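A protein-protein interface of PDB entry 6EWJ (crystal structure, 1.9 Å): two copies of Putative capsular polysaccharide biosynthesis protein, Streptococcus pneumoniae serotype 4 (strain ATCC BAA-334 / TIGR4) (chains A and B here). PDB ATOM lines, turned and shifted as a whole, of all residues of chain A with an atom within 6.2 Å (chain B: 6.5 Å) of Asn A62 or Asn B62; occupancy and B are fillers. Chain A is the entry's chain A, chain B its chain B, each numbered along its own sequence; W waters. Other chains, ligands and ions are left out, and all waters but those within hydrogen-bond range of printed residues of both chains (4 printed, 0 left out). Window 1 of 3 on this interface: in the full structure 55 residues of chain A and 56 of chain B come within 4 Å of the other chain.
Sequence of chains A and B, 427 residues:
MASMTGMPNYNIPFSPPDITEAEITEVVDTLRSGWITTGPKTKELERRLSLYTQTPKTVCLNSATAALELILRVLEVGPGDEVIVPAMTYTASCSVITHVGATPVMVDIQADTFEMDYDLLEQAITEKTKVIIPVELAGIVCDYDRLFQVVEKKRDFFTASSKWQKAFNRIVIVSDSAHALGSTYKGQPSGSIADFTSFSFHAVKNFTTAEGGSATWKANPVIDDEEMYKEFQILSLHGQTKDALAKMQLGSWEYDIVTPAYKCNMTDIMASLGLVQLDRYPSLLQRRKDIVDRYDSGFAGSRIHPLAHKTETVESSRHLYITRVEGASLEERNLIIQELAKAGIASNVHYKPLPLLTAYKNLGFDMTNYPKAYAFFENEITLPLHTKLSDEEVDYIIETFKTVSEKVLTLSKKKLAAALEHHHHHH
The side-chain amide oxygen (OD1) of Asn B62 sits at hydrogen-bond distance from the side-chain amide nitrogen (ND2) of Asn A62 (3.2 Å). The side-chain amino group (NZ) of Lys A263 lies within salt-bridge range of the side-chain carboxylate (OE2) of Glu B211. ND2 of Asn A265 is in hydrogen-bond range of OE2 of Glu B211, 2.9 Å away. OE2 of Glu A211 sits at hydrogen-bond distance from ND2 of Asn B265 (3.0 Å). OE2 of Glu A211 is in salt-bridge range of NZ of Lys B263 (2.9 Å).
The backbone carbonyl oxygen (O) of Glu B211 lies within hydrogen-bond range of the side-chain hydroxyl (OG1) of Thr B209, 2.9 Å away. The backbone NH (N) of Ala B66 lies within hydrogen-bond range of the side-chain hydroxyl (OG) of Ser B63 (2.8 Å). The side-chain hydroxyl of Ser A63 lies within hydrogen-bond range of the backbone NH of Ala A66, 2.8 Å away. NZ of Lys A263 sits at hydrogen-bond distance from OD1 of Asn A265 (2.9 Å). The backbone carbonyl oxygen of Asn B62 sits at hydrogen-bond distance from the backbone NH of Gly B212, at 3.2 Å. The backbone carbonyl oxygen (O) of Asn A62 is in hydrogen-bond range of the backbone NH (N) of Gly A212, at 3.2 Å.
Among the printed residues, merely in contact across the chains: Glu A211 with Thr B267 (3.3 Å), Lys A263 with Ser B63 (3.7 Å) and Ser A63 with Lys B263 (3.7 Å).
Of chain B, only Asn B62 (3.2 Å) comes within 4 Å of Asn A62. Of the printed residues of chain B, Lys A263 touches Ser B63 and Glu B211. Of the printed residues of chain A, Asn B62 touches Asn A62. Of the printed residues of chain A, Lys B263 touches Ser A63 and Glu A211. Of the printed residues of chain A, Thr B267 touches Glu A211. The nearest residue of chain B that does not touch Asn A62 is Lys B263 (4.7 Å). The nearest residue of chain A that does not touch Asn B62 is Lys A263 (4.7 Å).
Of the 18 printed residues of chain B, 6 touch a printed residue of chain A. Among the printed residues, Asp or Glu carboxylates within 4 Å of a Lys or Arg side-chain nitrogen of the other chain: Glu A211 with Lys B263 (2.9 Å) and Lys A263 with Glu B211 (2.9 Å).
Asn A62 touches its own counterpart, Asn B62. Ser A63 touches Lys B263, and with the chains exchanged Lys A263 touches Ser B63. Glu A211 touches Lys B263, and with the chains exchanged Lys A263 touches Glu B211. Glu A211 touches Asn B265, and with the chains exchanged Asn A265 touches Glu B211.
Water W1 lies within hydrogen-bond range of the side-chain hydroxyl (OG) of Ser A63 (2.5 Å), the side-chain amide oxygen (OD1) of Asn A62 (2.6 Å) and the backbone carbonyl oxygen (O) of Lys B263 (2.8 Å). Water W2 lies within hydrogen-bond range of ND2 of Asn B62, O of Lys A263 and OG of Ser B63. Water W4 lies within hydrogen-bond range of the side-chain amide oxygen of Asn B62 (2.9 Å), the side-chain amide nitrogen of Asn A62 (3.0 Å) and the backbone carbonyl oxygen of Lys B263 (3.3 Å). Water W3 bridges NZ of Lys B263 and OE2 of Glu A211.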
ATOM      1  N   CYS A  60      15.991  13.557 -12.011  1.00  0.00           N
ATOM      2  CA  CYS A  60      15.052  13.887 -10.954  1.00  0.00           C
ATOM      3  C   CYS A  60      15.662  15.056 -10.191  1.00  0.00           C
ATOM      4  O   CYS A  60      16.871  15.054  -9.894  1.00  0.00           O
ATOM      5  CB  CYS A  60      14.834  12.739 -10.007  1.00  0.00           C
ATOM      6  SG  CYS A  60      13.590  11.592 -10.589  1.00  0.00           S
ATOM      7  N   LEU A  61      14.832  16.077  -9.951  1.00  0.00           N
ATOM      8  CA  LEU A  61      15.300  17.326  -9.352  1.00  0.00           C
ATOM      9  C   LEU A  61      14.292  17.799  -8.300  1.00  0.00           C
ATOM     10  O   LEU A  61      13.261  17.134  -8.021  1.00  0.00           O
ATOM     11  CB  LEU A  61      15.457  18.360 -10.460  1.00  0.00           C
ATOM     12  CG  LEU A  61      16.390  18.076 -11.648  1.00  0.00           C
ATOM     13  CD1 LEU A  61      16.153  19.034 -12.790  1.00  0.00           C
ATOM     14  CD2 LEU A  61      17.810  18.133 -11.207  1.00  0.00           C
ATOM     15  N   ASN A  62      14.544  18.966  -7.709  1.00  0.00           N
ATOM     16  CA  ASN A  62      13.703  19.416  -6.565  1.00  0.00           C
ATOM     17  C   ASN A  62      12.428  20.179  -6.881  1.00  0.00           C
ATOM     18  O   ASN A  62      11.654  20.466  -5.969  1.00  0.00           O
ATOM     19  CB  ASN A  62      14.534  20.189  -5.507  1.00  0.00           C
ATOM     20  CG  ASN A  62      14.960  21.585  -5.968  1.00  0.00           C
ATOM     21  OD1 ASN A  62      14.488  22.119  -6.994  1.00  0.00           O
ATOM     22  ND2 ASN A  62      15.900  22.171  -5.227  1.00  0.00           N
ATOM     23  N   SER A  63      12.200  20.471  -8.165  1.00  0.00           N
ATOM     24  CA  SER A  63      10.976  21.108  -8.643  1.00  0.00           C
ATOM     25  C   SER A  63      10.923  21.001 -10.149  1.00  0.00           C
ATOM     26  O   SER A  63      11.976  20.753 -10.809  1.00  0.00           O
ATOM     27  CB  SER A  63      10.854  22.611  -8.239  1.00  0.00           C
ATOM     28  OG  SER A  63      11.718  23.432  -8.997  1.00  0.00           O
ATOM     29  N   ALA A  64       9.721  21.122 -10.702  1.00  0.00           N
ATOM     30  CA  ALA A  64       9.577  21.275 -12.125  1.00  0.00           C
ATOM     31  C   ALA A  64      10.218  22.560 -12.610  1.00  0.00           C
ATOM     32  O   ALA A  64      10.655  22.629 -13.775  1.00  0.00           O
ATOM     33  CB  ALA A  64       8.096  21.249 -12.525  1.00  0.00           C
ATOM     34  N   ALA A  66      12.895  24.034 -11.446  1.00  0.00           N
ATOM     35  CA  ALA A  66      14.293  23.659 -11.641  1.00  0.00           C
ATOM     36  C   ALA A  66      14.539  22.911 -12.947  1.00  0.00           C
ATOM     37  O   ALA A  66      15.523  23.194 -13.657  1.00  0.00           O
ATOM     38  CB  ALA A  66      14.819  22.868 -10.465  1.00  0.00           C
ATOM     39  N   GLU A 211       7.895  18.131  -2.629  1.00  0.00           N
ATOM     40  CA  GLU A 211       8.529  18.994  -3.620  1.00  0.00           C
ATOM     41  C   GLU A 211       9.388  18.088  -4.508  1.00  0.00           C
ATOM     42  O   GLU A 211      10.099  17.217  -4.023  1.00  0.00           O
ATOM     43  CB  GLU A 211       9.388  20.108  -2.973  1.00  0.00           C
ATOM     44  CG  GLU A 211       8.604  21.137  -2.145  1.00  0.00           C
ATOM     45  CD  GLU A 211       7.810  22.145  -2.966  1.00  0.00           C
ATOM     46  OE1 GLU A 211       7.948  22.193  -4.218  1.00  0.00           O
ATOM     47  OE2 GLU A 211       7.031  22.907  -2.359  1.00  0.00           O
ATOM     48  N   GLY A 212       9.320  18.306  -5.804  1.00  0.00           N
ATOM     49  CA  GLY A 212      10.148  17.578  -6.722  1.00  0.00           C
ATOM     50  C   GLY A 212       9.700  17.770  -8.154  1.00  0.00           C
ATOM     51  O   GLY A 212       8.655  18.377  -8.445  1.00  0.00           O
ATOM     52  N   GLY A 213      10.515  17.270  -9.064  1.00  0.00           N
ATOM     53  CA  GLY A 213      10.176  17.217 -10.440  1.00  0.00           C
ATOM     54  C   GLY A 213      11.275  16.551 -11.201  1.00  0.00           C
ATOM     55  O   GLY A 213      12.239  15.959 -10.606  1.00  0.00           O
ATOM     56  N   LYS A 263      21.845  24.188  -7.494  1.00  0.00           N
ATOM     57  CA  LYS A 263      21.707  23.311  -6.362  1.00  0.00           C
ATOM     58  C   LYS A 263      20.252  22.931  -6.353  1.00  0.00           C
ATOM     59  O   LYS A 263      19.433  23.558  -5.677  1.00  0.00           O
ATOM     60  CB  LYS A 263      22.184  24.058  -5.082  1.00  0.00           C
ATOM     61  CG  LYS A 263      22.100  23.277  -3.812  1.00  0.00           C
ATOM     62  CD  LYS A 263      22.763  21.896  -3.917  1.00  0.00           C
ATOM     63  CE  LYS A 263      22.681  21.129  -2.597  1.00  0.00           C
ATOM     64  NZ  LYS A 263      22.920  19.671  -2.756  1.00  0.00           N
ATOM     65  N   CYS A 264      19.908  21.893  -7.140  1.00  0.00           N
ATOM     66  CA  CYS A 264      18.540  21.462  -7.214  1.00  0.00           C
ATOM     67  C   CYS A 264      18.333  19.987  -7.388  1.00  0.00           C
ATOM     68  O   CYS A 264      17.322  19.564  -7.944  1.00  0.00           O
ATOM     69  CB  CYS A 264      17.818  22.241  -8.323  1.00  0.00           C
ATOM     70  SG  CYS A 264      18.635  22.173  -9.920  1.00  0.00           S
ATOM     71  N   ASN A 265      19.219  19.210  -6.798  1.00  0.00           N
ATOM     72  CA  ASN A 265      19.124  17.739  -6.756  1.00  0.00           C
ATOM     73  C   ASN A 265      17.988  17.253  -5.874  1.00  0.00           C
ATOM     74  O   ASN A 265      17.482  18.013  -5.022  1.00  0.00           O
ATOM     75  CB  ASN A 265      20.447  17.134  -6.242  1.00  0.00           C
ATOM     76  CG  ASN A 265      20.829  17.668  -4.882  1.00  0.00           C
ATOM     77  OD1 ASN A 265      20.952  18.905  -4.685  1.00  0.00           O
ATOM     78  ND2 ASN A 265      21.055  16.790  -3.927  1.00  0.00           N
ATOM     79  N   MET A 266      17.504  16.047  -6.190  1.00  0.00           N
ATOM     80  CA  MET A 266      16.474  15.317  -5.423  1.00  0.00           C
ATOM     81  C   MET A 266      17.086  14.428  -4.371  1.00  0.00           C
ATOM     82  O   MET A 266      18.082  13.709  -4.650  1.00  0.00           O
ATOM     83  CB  MET A 266      15.586  14.461  -6.356  1.00  0.00           C
ATOM     84  CG  MET A 266      14.464  13.807  -5.581  1.00  0.00           C
ATOM     85  SD  MET A 266      13.396  12.689  -6.481  1.00  0.00           S
ATOM     86  CE  MET A 266      12.360  13.979  -7.217  1.00  0.00           C
ATOM     87  N   CYS B  60      13.824  29.598   6.475  1.00  0.00           N
ATOM     88  CA  CYS B  60      14.315  28.268   6.172  1.00  0.00           C
ATOM     89  C   CYS B  60      14.096  28.048   4.667  1.00  0.00           C
ATOM     90  O   CYS B  60      12.980  28.296   4.150  1.00  0.00           O
ATOM     91  CB  CYS B  60      13.575  27.219   6.991  1.00  0.00           C
ATOM     92  SG  CYS B  60      14.282  27.084   8.670  1.00  0.00           S
ATOM     93  N   LEU B  61      15.117  27.527   4.009  1.00  0.00           N
ATOM     94  CA  LEU B  61      15.080  27.285   2.562  1.00  0.00           C
ATOM     95  C   LEU B  61      15.644  25.854   2.235  1.00  0.00           C
ATOM     96  O   LEU B  61      16.089  25.090   3.142  1.00  0.00           O
ATOM     97  CB  LEU B  61      15.898  28.362   1.901  1.00  0.00           C
ATOM     98  CG  LEU B  61      15.455  29.829   2.178  1.00  0.00           C
ATOM     99  CD1 LEU B  61      16.528  30.788   1.718  1.00  0.00           C
ATOM    100  CD2 LEU B  61      14.152  30.083   1.447  1.00  0.00           C
ATOM    101  N   ASN B  62      15.695  25.539   0.942  1.00  0.00           N
ATOM    102  CA  ASN B  62      16.158  24.190   0.545  1.00  0.00           C
ATOM    103  C   ASN B  62      17.671  23.922   0.474  1.00  0.00           C
ATOM    104  O   ASN B  62      18.076  22.783   0.251  1.00  0.00           O
ATOM    105  CB  ASN B  62      15.469  23.715  -0.739  1.00  0.00           C
ATOM    106  CG  ASN B  62      15.875  24.417  -1.970  1.00  0.00           C
ATOM    107  OD1 ASN B  62      15.188  24.302  -3.006  1.00  0.00           O
ATOM    108  ND2 ASN B  62      17.023  25.048  -1.945  1.00  0.00           N
ATOM    109  N   SER B  63      18.489  24.963   0.652  1.00  0.00           N
ATOM    110  CA  SER B  63      19.950  24.838   0.709  1.00  0.00           C
ATOM    111  C   SER B  63      20.529  26.155   1.255  1.00  0.00           C
ATOM    112  O   SER B  63      19.845  27.208   1.231  1.00  0.00           O
ATOM    113  CB  SER B  63      20.597  24.559  -0.682  1.00  0.00           C
ATOM    114  OG  SER B  63      20.585  25.719  -1.548  1.00  0.00           O
ATOM    115  N   ALA B  64      21.789  26.090   1.695  1.00  0.00           N
ATOM    116  CA  ALA B  64      22.553  27.281   2.045  1.00  0.00           C
ATOM    117  C   ALA B  64      22.880  28.099   0.823  1.00  0.00           C
ATOM    118  O   ALA B  64      22.932  29.324   0.896  1.00  0.00           O
ATOM    119  CB  ALA B  64      23.843  26.907   2.729  1.00  0.00           C
ATOM    120  N   THR B  65      23.088  27.438  -0.310  1.00  0.00           N
ATOM    121  CA  THR B  65      23.321  28.124  -1.567  1.00  0.00           C
ATOM    122  C   THR B  65      22.111  29.026  -1.916  1.00  0.00           C
ATOM    123  O   THR B  65      22.329  30.171  -2.323  1.00  0.00           O
ATOM    124  CB  THR B  65      23.595  27.153  -2.713  1.00  0.00           C
ATOM    125  OG1 THR B  65      24.704  26.334  -2.362  1.00  0.00           O
ATOM    126  CG2 THR B  65      23.947  27.868  -3.987  1.00  0.00           C
ATOM    127  N   ALA B  66      20.890  28.495  -1.792  1.00  0.00           N
ATOM    128  CA  ALA B  66      19.651  29.278  -2.000  1.00  0.00           C
ATOM    129  C   ALA B  66      19.592  30.459  -1.028  1.00  0.00           C
ATOM    130  O   ALA B  66      19.273  31.589  -1.447  1.00  0.00           O
ATOM    131  CB  ALA B  66      18.421  28.403  -1.829  1.00  0.00           C
ATOM    132  N   ALA B  67      19.953  30.228   0.244  1.00  0.00           N
ATOM    133  CA  ALA B  67      19.970  31.296   1.227  1.00  0.00           C
ATOM    134  C   ALA B  67      20.950  32.419   0.863  1.00  0.00           C
ATOM    135  O   ALA B  67      20.594  33.592   0.924  1.00  0.00           O
ATOM    136  CB  ALA B  67      20.241  30.768   2.608  1.00  0.00           C
ATOM    137  N   THR B 209      18.995  18.370   7.509  1.00  0.00           N
ATOM    138  CA  THR B 209      17.684  18.037   7.065  1.00  0.00           C
ATOM    139  C   THR B 209      17.831  17.364   5.719  1.00  0.00           C
ATOM    140  O   THR B 209      16.897  17.399   4.917  1.00  0.00           O
ATOM    141  CB  THR B 209      16.777  19.306   6.974  1.00  0.00           C
ATOM    142  OG1 THR B 209      17.322  20.230   6.018  1.00  0.00           O
ATOM    143  CG2 THR B 209      16.647  19.971   8.305  1.00  0.00           C
ATOM    144  N   GLU B 211      18.696  17.898   2.749  1.00  0.00           N
ATOM    145  CA  GLU B 211      18.979  19.132   2.009  1.00  0.00           C
ATOM    146  C   GLU B 211      18.221  20.264   2.731  1.00  0.00           C
ATOM    147  O   GLU B 211      17.090  20.089   3.153  1.00  0.00           O
ATOM    148  CB  GLU B 211      18.567  19.044   0.550  1.00  0.00           C
ATOM    149  CG  GLU B 211      19.324  18.042  -0.298  1.00  0.00           C
ATOM    150  CD  GLU B 211      20.747  18.468  -0.646  1.00  0.00           C
ATOM    151  OE1 GLU B 211      21.138  19.653  -0.395  1.00  0.00           O
ATOM    152  OE2 GLU B 211      21.517  17.619  -1.189  1.00  0.00           O
ATOM    153  N   GLY B 212      18.910  21.365   2.975  1.00  0.00           N
ATOM    154  CA  GLY B 212      18.263  22.518   3.579  1.00  0.00           C
ATOM    155  C   GLY B 212      19.254  23.569   3.985  1.00  0.00           C
ATOM    156  O   GLY B 212      20.490  23.374   3.929  1.00  0.00           O
ATOM    157  N   GLY B 213      18.716  24.693   4.389  1.00  0.00           N
ATOM    158  CA  GLY B 213      19.523  25.761   4.967  1.00  0.00           C
ATOM    159  C   GLY B 213      18.623  26.902   5.356  1.00  0.00           C
ATOM    160  O   GLY B 213      17.363  26.787   5.294  1.00  0.00           O
ATOM    161  N   SER B 214      19.261  28.010   5.733  1.00  0.00           N
ATOM    162  CA  SER B 214      18.541  29.150   6.182  1.00  0.00           C
ATOM    163  C   SER B 214      19.329  30.436   6.038  1.00  0.00           C
ATOM    164  O   SER B 214      20.560  30.427   5.938  1.00  0.00           O
ATOM    165  CB  SER B 214      18.179  28.988   7.675  1.00  0.00           C
ATOM    166  OG  SER B 214      19.304  29.108   8.526  1.00  0.00           O
ATOM    167  N   LYS B 263      12.271  29.177  -6.543  1.00  0.00           N
ATOM    168  CA  LYS B 263      11.555  28.077  -5.980  1.00  0.00           C
ATOM    169  C   LYS B 263      12.510  27.320  -5.069  1.00  0.00           C
ATOM    170  O   LYS B 263      13.233  26.424  -5.499  1.00  0.00           O
ATOM    171  CB  LYS B 263      11.054  27.204  -7.151  1.00  0.00           C
ATOM    172  CG  LYS B 263      10.221  25.997  -6.787  1.00  0.00           C
ATOM    173  CD  LYS B 263       9.107  26.316  -5.804  1.00  0.00           C
ATOM    174  CE  LYS B 263       8.322  25.047  -5.440  1.00  0.00           C
ATOM    175  NZ  LYS B 263       7.512  25.181  -4.173  1.00  0.00           N
ATOM    176  N   CYS B 264      12.555  27.730  -3.825  1.00  0.00           N
ATOM    177  CA  CYS B 264      13.548  27.115  -2.901  1.00  0.00           C
ATOM    178  C   CYS B 264      13.103  27.035  -1.487  1.00  0.00           C
ATOM    179  O   CYS B 264      13.916  27.131  -0.558  1.00  0.00           O
ATOM    180  CB  CYS B 264      14.885  27.849  -3.033  1.00  0.00           C
ATOM    181  SG  CYS B 264      14.826  29.688  -2.805  1.00  0.00           S
ATOM    182  N   ASN B 265      11.800  26.922  -1.309  1.00  0.00           N
ATOM    183  CA  ASN B 265      11.197  26.762   0.018  1.00  0.00           C
ATOM    184  C   ASN B 265      11.581  25.434   0.664  1.00  0.00           C
ATOM    185  O   ASN B 265      11.938  24.494  -0.059  1.00  0.00           O
ATOM    186  CB  ASN B 265       9.692  26.885  -0.064  1.00  0.00           C
ATOM    187  CG  ASN B 265       9.087  25.901  -1.072  1.00  0.00           C
ATOM    188  OD1 ASN B 265       9.458  25.924  -2.258  1.00  0.00           O
ATOM    189  ND2 ASN B 265       8.153  25.082  -0.637  1.00  0.00           N
ATOM    190  N   MET B 266      11.534  25.407   2.001  1.00  0.00           N
ATOM    191  CA  MET B 266      11.696  24.209   2.793  1.00  0.00           C
ATOM    192  C   MET B 266      10.367  23.502   3.044  1.00  0.00           C
ATOM    193  O   MET B 266       9.362  24.142   3.407  1.00  0.00           O
ATOM    194  CB  MET B 266      12.364  24.519   4.171  1.00  0.00           C
ATOM    195  CG  MET B 266      12.656  23.232   4.941  1.00  0.00           C
ATOM    196  SD  MET B 266      13.392  23.471   6.580  1.00  0.00           S
ATOM    197  CE  MET B 266      15.054  23.713   6.027  1.00  0.00           C
ATOM    198  N   THR B 267      10.385  22.176   2.912  1.00  0.00           N
ATOM    199  CA  THR B 267       9.225  21.380   3.217  1.00  0.00           C
ATOM    200  C   THR B 267       9.170  21.032   4.693  1.00  0.00           C
ATOM    201  O   THR B 267      10.173  21.005   5.373  1.00  0.00           O
ATOM    202  CB  THR B 267       9.208  20.054   2.455  1.00  0.00           C
ATOM    203  OG1 THR B 267      10.320  19.254   2.874  1.00  0.00           O
ATOM    204  CG2 THR B 267       9.271  20.201   0.931  1.00  0.00           C
HETATM  205  O   HOH W   1      13.437  24.425  -7.504  1.00  0.00           O
HETATM  206  O   HOH W   2      19.007  25.224  -3.665  1.00  0.00           O
HETATM  207  O   HOH W   3       4.896  25.190  -2.742  1.00  0.00           O
HETATM  208  O   HOH W   4      16.306  25.145  -5.495  1.00  0.00           O
